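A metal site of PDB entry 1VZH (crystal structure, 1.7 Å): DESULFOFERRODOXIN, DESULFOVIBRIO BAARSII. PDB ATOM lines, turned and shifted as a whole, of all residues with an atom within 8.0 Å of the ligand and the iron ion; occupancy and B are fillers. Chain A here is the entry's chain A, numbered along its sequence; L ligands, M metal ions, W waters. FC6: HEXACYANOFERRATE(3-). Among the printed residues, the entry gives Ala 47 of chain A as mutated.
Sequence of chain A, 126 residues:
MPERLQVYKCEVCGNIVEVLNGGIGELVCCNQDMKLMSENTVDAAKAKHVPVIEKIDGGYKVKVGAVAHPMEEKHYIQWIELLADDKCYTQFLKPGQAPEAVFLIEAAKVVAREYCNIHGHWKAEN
A nitrogen (N23) of the ligand sits at hydrogen-bond distance from the backbone NH (N) of Ala 45 (3.3 Å). A nitrogen (N25) of the ligand lies within hydrogen-bond range of the side-chain amino group of Lys 48, at 3.1 Å.
NE1 of Trp 122 is in hydrogen-bond range of O of His 119, at 2.9 Å. The backbone NH (N) of His 69 lies within hydrogen-bond range of the backbone carbonyl oxygen (O) of Val 64 (2.9 Å). A ring nitrogen (ND1) of His 49 sits at hydrogen-bond distance from the backbone carbonyl oxygen (O) of Ala 45, 2.7 Å away. O of His 49 sits close to OE2 of Glu 114 (2.6 Å). SG of Cys 116 sits close to N of Ile 118. The side-chain carboxylate (OE1) of Glu 114 is in hydrogen-bond range of the backbone NH (N) of Cys 116 (3.3 Å).
Residues that only touch the ligand: Ala 44 (3.7 Å) and Pro 70 (3.7 Å). Hydrophobic or aromatic side chains within 4 Å of the ligand: Ala 44, Ala 45, His 49, His 69, Pro 70, His 75 and His 119. Within 4 Å of the ligand: Ala 44, Ala 45, Lys 48, His 49, His 69, Pro 70, His 75 and His 119. The nearest printed residue that does not touch the ligand is Cys 116 (5.1 Å).
Five residues have an atom within 4 Å of the iron ion: His 49, His 69, His 75, Cys 116 and His 119. Along chain A the residues within 4 Å of the iron ion span positions 49 to 119. The nearest printed residue that does not touch the iron ion is Ile 118 (4.9 Å).
ND1 of His 119 binds the iron ion (2.2 Å). NE2 of His 75 binds the iron ion (2.2 Å). The iron ion is bound by a ring nitrogen (NE2) of His 69, 2.2 Å away. The iron ion is bound by NE2 of His 49 (2.2 Å). A nitrogen (N24) of the ligand is bound to the iron ion, at 2.4 Å. The iron ion is bound by the side-chain sulfur (SG) of Cys 116 (2.7 Å). The iron ion has six donor atoms within binding distance.
Water W1 lies within hydrogen-bond range of a ring nitrogen (NE2) of His 119 (2.9 Å) and a nitrogen (N21) of the ligand (3.3 Å).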
ATOM      1  N   VAL A  42     -14.536 -13.294  18.020  1.00  0.00           N
ATOM      2  CA  VAL A  42     -13.272 -12.908  17.391  1.00  0.00           C
ATOM      3  C   VAL A  42     -12.124 -13.836  17.763  1.00  0.00           C
ATOM      4  O   VAL A  42     -11.994 -14.268  18.910  1.00  0.00           O
ATOM      5  CB  VAL A  42     -12.891 -11.456  17.750  1.00  0.00           C
ATOM      6  CG1 VAL A  42     -11.501 -11.128  17.219  1.00  0.00           C
ATOM      7  CG2 VAL A  42     -13.915 -10.490  17.160  1.00  0.00           C
ATOM      8  N   ASP A  43     -11.280 -14.133  16.775  1.00  0.00           N
ATOM      9  CA  ASP A  43     -10.121 -14.990  16.985  1.00  0.00           C
ATOM     10  C   ASP A  43      -9.004 -14.189  17.648  1.00  0.00           C
ATOM     11  O   ASP A  43      -8.092 -13.706  16.985  1.00  0.00           O
ATOM     12  CB  ASP A  43      -9.633 -15.538  15.640  1.00  0.00           C
ATOM     13  CG  ASP A  43      -8.531 -16.572  15.794  1.00  0.00           C
ATOM     14  OD1 ASP A  43      -7.483 -16.259  16.379  1.00  0.00           O
ATOM     15  OD2 ASP A  43      -8.724 -17.709  15.308  1.00  0.00           O
ATOM     16  N   ALA A  44      -9.088 -14.035  18.966  1.00  0.00           N
ATOM     17  CA  ALA A  44      -8.077 -13.294  19.727  1.00  0.00           C
ATOM     18  C   ALA A  44      -7.845 -13.992  21.064  1.00  0.00           C
ATOM     19  O   ALA A  44      -8.656 -14.821  21.485  1.00  0.00           O
ATOM     20  CB  ALA A  44      -8.534 -11.849  19.947  1.00  0.00           C
ATOM     21  N   ALA A  45      -6.748 -13.651  21.722  1.00  0.00           N
ATOM     22  CA  ALA A  45      -6.398 -14.272  23.007  1.00  0.00           C
ATOM     23  C   ALA A  45      -7.461 -14.035  24.075  1.00  0.00           C
ATOM     24  O   ALA A  45      -7.763 -12.893  24.425  1.00  0.00           O
ATOM     25  CB  ALA A  45      -5.055 -13.754  23.479  1.00  0.00           C
ATOM     26  N   LYS A  46      -8.014 -15.119  24.594  1.00  0.00           N
ATOM     27  CA  LYS A  46      -9.037 -15.026  25.627  1.00  0.00           C
ATOM     28  C   LYS A  46      -8.425 -14.526  26.940  1.00  0.00           C
ATOM     29  O   LYS A  46      -9.086 -13.849  27.711  1.00  0.00           O
ATOM     30  CB  LYS A  46      -9.693 -16.387  25.864  1.00  0.00           C
ATOM     31  CG  LYS A  46     -10.413 -16.941  24.641  1.00  0.00           C
ATOM     32  CD  LYS A  46     -11.124 -18.248  24.963  1.00  0.00           C
ATOM     33  CE  LYS A  46     -10.171 -19.285  25.538  1.00  0.00           C
ATOM     34  NZ  LYS A  46      -9.073 -19.635  24.594  1.00  0.00           N
ATOM     35  N   ALA A  47      -7.163 -14.871  27.166  1.00  0.00           N
ATOM     36  CA  ALA A  47      -6.461 -14.458  28.390  1.00  0.00           C
ATOM     37  C   ALA A  47      -6.492 -12.950  28.609  1.00  0.00           C
ATOM     38  O   ALA A  47      -6.585 -12.477  29.747  1.00  0.00           O
ATOM     39  CB  ALA A  47      -5.018 -14.951  28.354  1.00  0.00           C
ATOM     40  N   LYS A  48      -6.417 -12.186  27.517  1.00  0.00           N
ATOM     41  CA  LYS A  48      -6.434 -10.736  27.630  1.00  0.00           C
ATOM     42  C   LYS A  48      -7.788 -10.092  27.324  1.00  0.00           C
ATOM     43  O   LYS A  48      -7.976  -8.910  27.621  1.00  0.00           O
ATOM     44  CB  LYS A  48      -5.376 -10.110  26.711  1.00  0.00           C
ATOM     45  CG  LYS A  48      -3.942 -10.391  27.115  1.00  0.00           C
ATOM     46  CD  LYS A  48      -2.972  -9.553  26.301  1.00  0.00           C
ATOM     47  CE  LYS A  48      -1.522  -9.802  26.713  1.00  0.00           C
ATOM     48  NZ  LYS A  48      -0.590  -8.976  25.909  1.00  0.00           N
ATOM     49  N   HIS A  49      -8.715 -10.849  26.749  1.00  0.00           N
ATOM     50  CA  HIS A  49     -10.009 -10.283  26.389  1.00  0.00           C
ATOM     51  C   HIS A  49     -11.236 -10.719  27.175  1.00  0.00           C
ATOM     52  O   HIS A  49     -12.199  -9.961  27.283  1.00  0.00           O
ATOM     53  CB  HIS A  49     -10.287 -10.516  24.901  1.00  0.00           C
ATOM     54  CG  HIS A  49      -9.310  -9.813  24.001  1.00  0.00           C
ATOM     55  ND1 HIS A  49      -8.195 -10.447  23.496  1.00  0.00           N
ATOM     56  CD2 HIS A  49      -9.268  -8.550  23.547  1.00  0.00           C
ATOM     57  CE1 HIS A  49      -7.508  -9.586  22.758  1.00  0.00           C
ATOM     58  NE2 HIS A  49      -8.134  -8.424  22.777  1.00  0.00           N
ATOM     59  N   VAL A  64      -9.912  -6.875  32.712  1.00  0.00           N
ATOM     60  CA  VAL A  64      -9.784  -7.391  31.351  1.00  0.00           C
ATOM     61  C   VAL A  64      -8.304  -7.568  31.027  1.00  0.00           C
ATOM     62  O   VAL A  64      -7.599  -6.591  30.779  1.00  0.00           O
ATOM     63  CB  VAL A  64     -10.400  -6.396  30.329  1.00  0.00           C
ATOM     64  CG1 VAL A  64     -10.242  -6.930  28.912  1.00  0.00           C
ATOM     65  CG2 VAL A  64     -11.870  -6.154  30.649  1.00  0.00           C
ATOM     66  N   VAL A  67      -5.078 -11.792  32.014  1.00  0.00           N
ATOM     67  CA  VAL A  67      -3.804 -11.129  31.806  1.00  0.00           C
ATOM     68  C   VAL A  67      -4.189  -9.709  31.412  1.00  0.00           C
ATOM     69  O   VAL A  67      -5.007  -9.518  30.517  1.00  0.00           O
ATOM     70  CB  VAL A  67      -3.005 -11.785  30.655  1.00  0.00           C
ATOM     71  CG1 VAL A  67      -1.721 -11.003  30.406  1.00  0.00           C
ATOM     72  CG2 VAL A  67      -2.689 -13.232  30.991  1.00  0.00           C
ATOM     73  N   ALA A  68      -3.617  -8.720  32.089  1.00  0.00           N
ATOM     74  CA  ALA A  68      -3.922  -7.321  31.804  1.00  0.00           C
ATOM     75  C   ALA A  68      -3.824  -6.968  30.326  1.00  0.00           C
ATOM     76  O   ALA A  68      -2.785  -7.164  29.689  1.00  0.00           O
ATOM     77  CB  ALA A  68      -3.005  -6.423  32.607  1.00  0.00           C
ATOM     78  N   HIS A  69      -4.920  -6.445  29.766  1.00  0.00           N
ATOM     79  CA  HIS A  69      -4.965  -6.061  28.360  1.00  0.00           C
ATOM     80  C   HIS A  69      -4.285  -4.704  28.166  1.00  0.00           C
ATOM     81  O   HIS A  69      -4.321  -3.840  29.054  1.00  0.00           O
ATOM     82  CB  HIS A  69      -6.421  -5.990  27.883  1.00  0.00           C
ATOM     83  CG  HIS A  69      -6.578  -5.691  26.421  1.00  0.00           C
ATOM     84  ND1 HIS A  69      -6.418  -4.426  25.900  1.00  0.00           N
ATOM     85  CD2 HIS A  69      -6.905  -6.493  25.377  1.00  0.00           C
ATOM     86  CE1 HIS A  69      -6.626  -4.460  24.593  1.00  0.00           C
ATOM     87  NE2 HIS A  69      -6.928  -5.701  24.248  1.00  0.00           N
ATOM     88  N   PRO A  70      -3.651  -4.496  27.004  1.00  0.00           N
ATOM     89  CA  PRO A  70      -2.973  -3.225  26.723  1.00  0.00           C
ATOM     90  C   PRO A  70      -3.938  -2.034  26.734  1.00  0.00           C
ATOM     91  O   PRO A  70      -5.118  -2.183  26.413  1.00  0.00           O
ATOM     92  CB  PRO A  70      -2.386  -3.444  25.337  1.00  0.00           C
ATOM     93  CG  PRO A  70      -2.137  -4.916  25.307  1.00  0.00           C
ATOM     94  CD  PRO A  70      -3.373  -5.478  25.941  1.00  0.00           C
ATOM     95  N   GLU A  72      -3.142   1.142  25.143  1.00  0.00           N
ATOM     96  CA  GLU A  72      -2.354   2.033  24.297  1.00  0.00           C
ATOM     97  C   GLU A  72      -3.250   2.845  23.378  1.00  0.00           C
ATOM     98  O   GLU A  72      -4.381   2.454  23.087  1.00  0.00           O
ATOM     99  CB  GLU A  72      -1.388   1.198  23.449  1.00  0.00           C
ATOM    100  CG  GLU A  72      -0.491   0.273  24.251  1.00  0.00           C
ATOM    101  CD  GLU A  72       0.441  -0.552  23.366  1.00  0.00           C
ATOM    102  OE1 GLU A  72       1.163   0.058  22.553  1.00  0.00           O
ATOM    103  OE2 GLU A  72       0.438  -1.788  23.485  1.00  0.00           O
ATOM    104  N   HIS A  75      -4.542   0.638  20.702  1.00  0.00           N
ATOM    105  CA  HIS A  75      -5.056  -0.667  21.105  1.00  0.00           C
ATOM    106  C   HIS A  75      -5.405  -0.640  22.586  1.00  0.00           C
ATOM    107  O   HIS A  75      -4.531  -0.748  23.444  1.00  0.00           O
ATOM    108  CB  HIS A  75      -3.999  -1.749  20.859  1.00  0.00           C
ATOM    109  CG  HIS A  75      -4.466  -3.125  21.178  1.00  0.00           C
ATOM    110  ND1 HIS A  75      -3.601  -4.169  21.427  1.00  0.00           N
ATOM    111  CD2 HIS A  75      -5.717  -3.648  21.285  1.00  0.00           C
ATOM    112  CE1 HIS A  75      -4.298  -5.268  21.673  1.00  0.00           C
ATOM    113  NE2 HIS A  75      -5.584  -4.978  21.586  1.00  0.00           N
ATOM    114  N   TYR A  76      -6.698  -0.502  22.889  1.00  0.00           N
ATOM    115  CA  TYR A  76      -7.129  -0.438  24.274  1.00  0.00           C
ATOM    116  C   TYR A  76      -8.569  -0.894  24.447  1.00  0.00           C
ATOM    117  O   TYR A  76      -9.275  -1.126  23.466  1.00  0.00           O
ATOM    118  CB  TYR A  76      -7.011   1.003  24.793  1.00  0.00           C
ATOM    119  CG  TYR A  76      -7.924   1.999  24.095  1.00  0.00           C
ATOM    120  CD1 TYR A  76      -7.691   2.385  22.780  1.00  0.00           C
ATOM    121  CD2 TYR A  76      -9.009   2.562  24.768  1.00  0.00           C
ATOM    122  CE1 TYR A  76      -8.529   3.308  22.142  1.00  0.00           C
ATOM    123  CE2 TYR A  76      -9.846   3.488  24.144  1.00  0.00           C
ATOM    124  CZ  TYR A  76      -9.599   3.848  22.832  1.00  0.00           C
ATOM    125  OH  TYR A  76     -10.425   4.769  22.216  1.00  0.00           O
ATOM    126  N   ILE A  77      -8.988  -1.016  25.697  1.00  0.00           N
ATOM    127  CA  ILE A  77     -10.357  -1.424  26.017  1.00  0.00           C
ATOM    128  C   ILE A  77     -11.134  -0.120  26.090  1.00  0.00           C
ATOM    129  O   ILE A  77     -10.839   0.745  26.910  1.00  0.00           O
ATOM    130  CB  ILE A  77     -10.421  -2.157  27.390  1.00  0.00           C
ATOM    131  CG1 ILE A  77      -9.475  -3.351  27.380  1.00  0.00           C
ATOM    132  CG2 ILE A  77     -11.855  -2.610  27.676  1.00  0.00           C
ATOM    133  CD1 ILE A  77      -9.702  -4.313  26.229  1.00  0.00           C
ATOM    134  N   GLU A 114     -16.790  -6.267  27.646  1.00  0.00           N
ATOM    135  CA  GLU A 114     -15.739  -5.301  27.382  1.00  0.00           C
ATOM    136  C   GLU A 114     -15.577  -5.238  25.885  1.00  0.00           C
ATOM    137  O   GLU A 114     -15.803  -6.238  25.191  1.00  0.00           O
ATOM    138  CB  GLU A 114     -14.419  -5.738  28.029  1.00  0.00           C
ATOM    139  CG  GLU A 114     -13.815  -7.020  27.442  1.00  0.00           C
ATOM    140  CD  GLU A 114     -12.851  -6.780  26.286  1.00  0.00           C
ATOM    141  OE1 GLU A 114     -12.783  -5.644  25.774  1.00  0.00           O
ATOM    142  OE2 GLU A 114     -12.165  -7.743  25.890  1.00  0.00           O
ATOM    143  N   TYR A 115     -15.219  -4.068  25.386  1.00  0.00           N
ATOM    144  CA  TYR A 115     -15.019  -3.901  23.957  1.00  0.00           C
ATOM    145  C   TYR A 115     -13.618  -3.358  23.679  1.00  0.00           C
ATOM    146  O   TYR A 115     -13.226  -2.316  24.188  1.00  0.00           O
ATOM    147  CB  TYR A 115     -16.070  -2.954  23.371  1.00  0.00           C
ATOM    148  CG  TYR A 115     -15.950  -2.818  21.871  1.00  0.00           C
ATOM    149  CD1 TYR A 115     -15.119  -1.849  21.297  1.00  0.00           C
ATOM    150  CD2 TYR A 115     -16.642  -3.680  21.018  1.00  0.00           C
ATOM    151  CE1 TYR A 115     -14.978  -1.744  19.908  1.00  0.00           C
ATOM    152  CE2 TYR A 115     -16.511  -3.576  19.630  1.00  0.00           C
ATOM    153  CZ  TYR A 115     -15.677  -2.617  19.087  1.00  0.00           C
ATOM    154  OH  TYR A 115     -15.520  -2.541  17.723  1.00  0.00           O
ATOM    155  N   CYS A 116     -12.864  -4.119  22.882  1.00  0.00           N
ATOM    156  CA  CYS A 116     -11.507  -3.732  22.487  1.00  0.00           C
ATOM    157  C   CYS A 116     -11.600  -3.101  21.092  1.00  0.00           C
ATOM    158  O   CYS A 116     -12.239  -3.671  20.192  1.00  0.00           O
ATOM    159  CB  CYS A 116     -10.617  -4.970  22.443  1.00  0.00           C
ATOM    160  SG  CYS A 116      -8.957  -4.675  21.745  1.00  0.00           S
ATOM    161  N   ASN A 117     -10.980  -1.941  20.903  1.00  0.00           N
ATOM    162  CA  ASN A 117     -11.066  -1.254  19.621  1.00  0.00           C
ATOM    163  C   ASN A 117     -10.550  -2.110  18.460  1.00  0.00           C
ATOM    164  O   ASN A 117     -10.939  -1.903  17.307  1.00  0.00           O
ATOM    165  CB  ASN A 117     -10.299   0.083  19.671  1.00  0.00           C
ATOM    166  CG  ASN A 117      -8.799  -0.103  19.685  1.00  0.00           C
ATOM    167  OD1 ASN A 117      -8.253  -0.862  20.478  1.00  0.00           O
ATOM    168  ND2 ASN A 117      -8.109   0.622  18.811  1.00  0.00           N
ATOM    169  N   ILE A 118      -9.694  -3.074  18.768  1.00  0.00           N
ATOM    170  CA  ILE A 118      -9.157  -3.950  17.738  1.00  0.00           C
ATOM    171  C   ILE A 118      -9.795  -5.327  17.712  1.00  0.00           C
ATOM    172  O   ILE A 118     -10.193  -5.811  16.647  1.00  0.00           O
ATOM    173  CB  ILE A 118      -7.627  -4.142  17.917  1.00  0.00           C
ATOM    174  CG1 ILE A 118      -6.912  -2.798  17.782  1.00  0.00           C
ATOM    175  CG2 ILE A 118      -7.094  -5.130  16.870  1.00  0.00           C
ATOM    176  CD1 ILE A 118      -7.142  -2.115  16.447  1.00  0.00           C
ATOM    177  N   HIS A 119      -9.916  -5.964  18.877  1.00  0.00           N
ATOM    178  CA  HIS A 119     -10.451  -7.319  18.937  1.00  0.00           C
ATOM    179  C   HIS A 119     -11.907  -7.550  19.275  1.00  0.00           C
ATOM    180  O   HIS A 119     -12.302  -8.671  19.616  1.00  0.00           O
ATOM    181  CB  HIS A 119      -9.562  -8.146  19.860  1.00  0.00           C
ATOM    182  CG  HIS A 119      -8.117  -8.129  19.470  1.00  0.00           C
ATOM    183  ND1 HIS A 119      -7.164  -7.428  20.175  1.00  0.00           N
ATOM    184  CD2 HIS A 119      -7.484  -8.662  18.398  1.00  0.00           C
ATOM    185  CE1 HIS A 119      -5.996  -7.526  19.562  1.00  0.00           C
ATOM    186  NE2 HIS A 119      -6.162  -8.272  18.482  1.00  0.00           N
ATOM    187  N   GLY A 120     -12.714  -6.496  19.210  1.00  0.00           N
ATOM    188  CA  GLY A 120     -14.135  -6.658  19.442  1.00  0.00           C
ATOM    189  C   GLY A 120     -14.739  -6.781  20.834  1.00  0.00           C
ATOM    190  O   GLY A 120     -14.153  -6.418  21.854  1.00  0.00           O
ATOM    191  N   TRP A 122     -16.442  -8.852  24.016  1.00  0.00           N
ATOM    192  CA  TRP A 122     -16.252 -10.051  24.825  1.00  0.00           C
ATOM    193  C   TRP A 122     -17.090 -10.014  26.097  1.00  0.00           C
ATOM    194  O   TRP A 122     -17.403  -8.936  26.601  1.00  0.00           O
ATOM    195  CB  TRP A 122     -14.795 -10.222  25.217  1.00  0.00           C
ATOM    196  CG  TRP A 122     -13.902 -10.379  24.048  1.00  0.00           C
ATOM    197  CD1 TRP A 122     -13.493  -9.401  23.192  1.00  0.00           C
ATOM    198  CD2 TRP A 122     -13.341 -11.608  23.568  1.00  0.00           C
ATOM    199  NE1 TRP A 122     -12.711  -9.946  22.210  1.00  0.00           N
ATOM    200  CE2 TRP A 122     -12.601 -11.295  22.415  1.00  0.00           C
ATOM    201  CE3 TRP A 122     -13.404 -12.936  24.004  1.00  0.00           C
ATOM    202  CZ2 TRP A 122     -11.912 -12.268  21.676  1.00  0.00           C
ATOM    203  CZ3 TRP A 122     -12.723 -13.915  23.274  1.00  0.00           C
ATOM    204  CH2 TRP A 122     -11.989 -13.567  22.122  1.00  0.00           C
HETATM  205  N24 FC6 L   1      -5.136  -7.861  22.857  1.00  0.00           N
HETATM  206  C24 FC6 L   1      -4.266  -8.515  22.441  1.00  0.00           C
HETATM  207 FE2  FC6 L   1      -2.827  -9.604  21.741  1.00  0.00          FE
HETATM  208  C21 FC6 L   1      -1.604  -8.372  22.597  1.00  0.00           C
HETATM  209  N25 FC6 L   1      -0.872  -7.620  23.115  1.00  0.00           N
HETATM  210  C22 FC6 L   1      -2.832 -10.930  23.063  1.00  0.00           C
HETATM  211  N22 FC6 L   1      -2.831 -11.752  23.889  1.00  0.00           N
HETATM  212  C26 FC6 L   1      -2.803  -8.394  20.258  1.00  0.00           C
HETATM  213  N21 FC6 L   1      -2.784  -7.661  19.352  1.00  0.00           N
HETATM  214  C23 FC6 L   1      -4.071 -10.729  20.804  1.00  0.00           C
HETATM  215  N23 FC6 L   1      -4.836 -11.413  20.241  1.00  0.00           N
HETATM  216  C11 FC6 L   1      -1.370 -10.572  20.964  1.00  0.00           C
HETATM  217  N11 FC6 L   1      -0.482 -11.167  20.488  1.00  0.00           N
HETATM  218 FE    FE M   1      -7.061  -6.544  22.173  1.00  0.00          FE
HETATM  219  O   HOH W   1      -4.077  -8.817  16.488  1.00  0.00           O
HETATM  220  O   HOH W   2      -2.213 -13.775  25.899  1.00  0.00           O
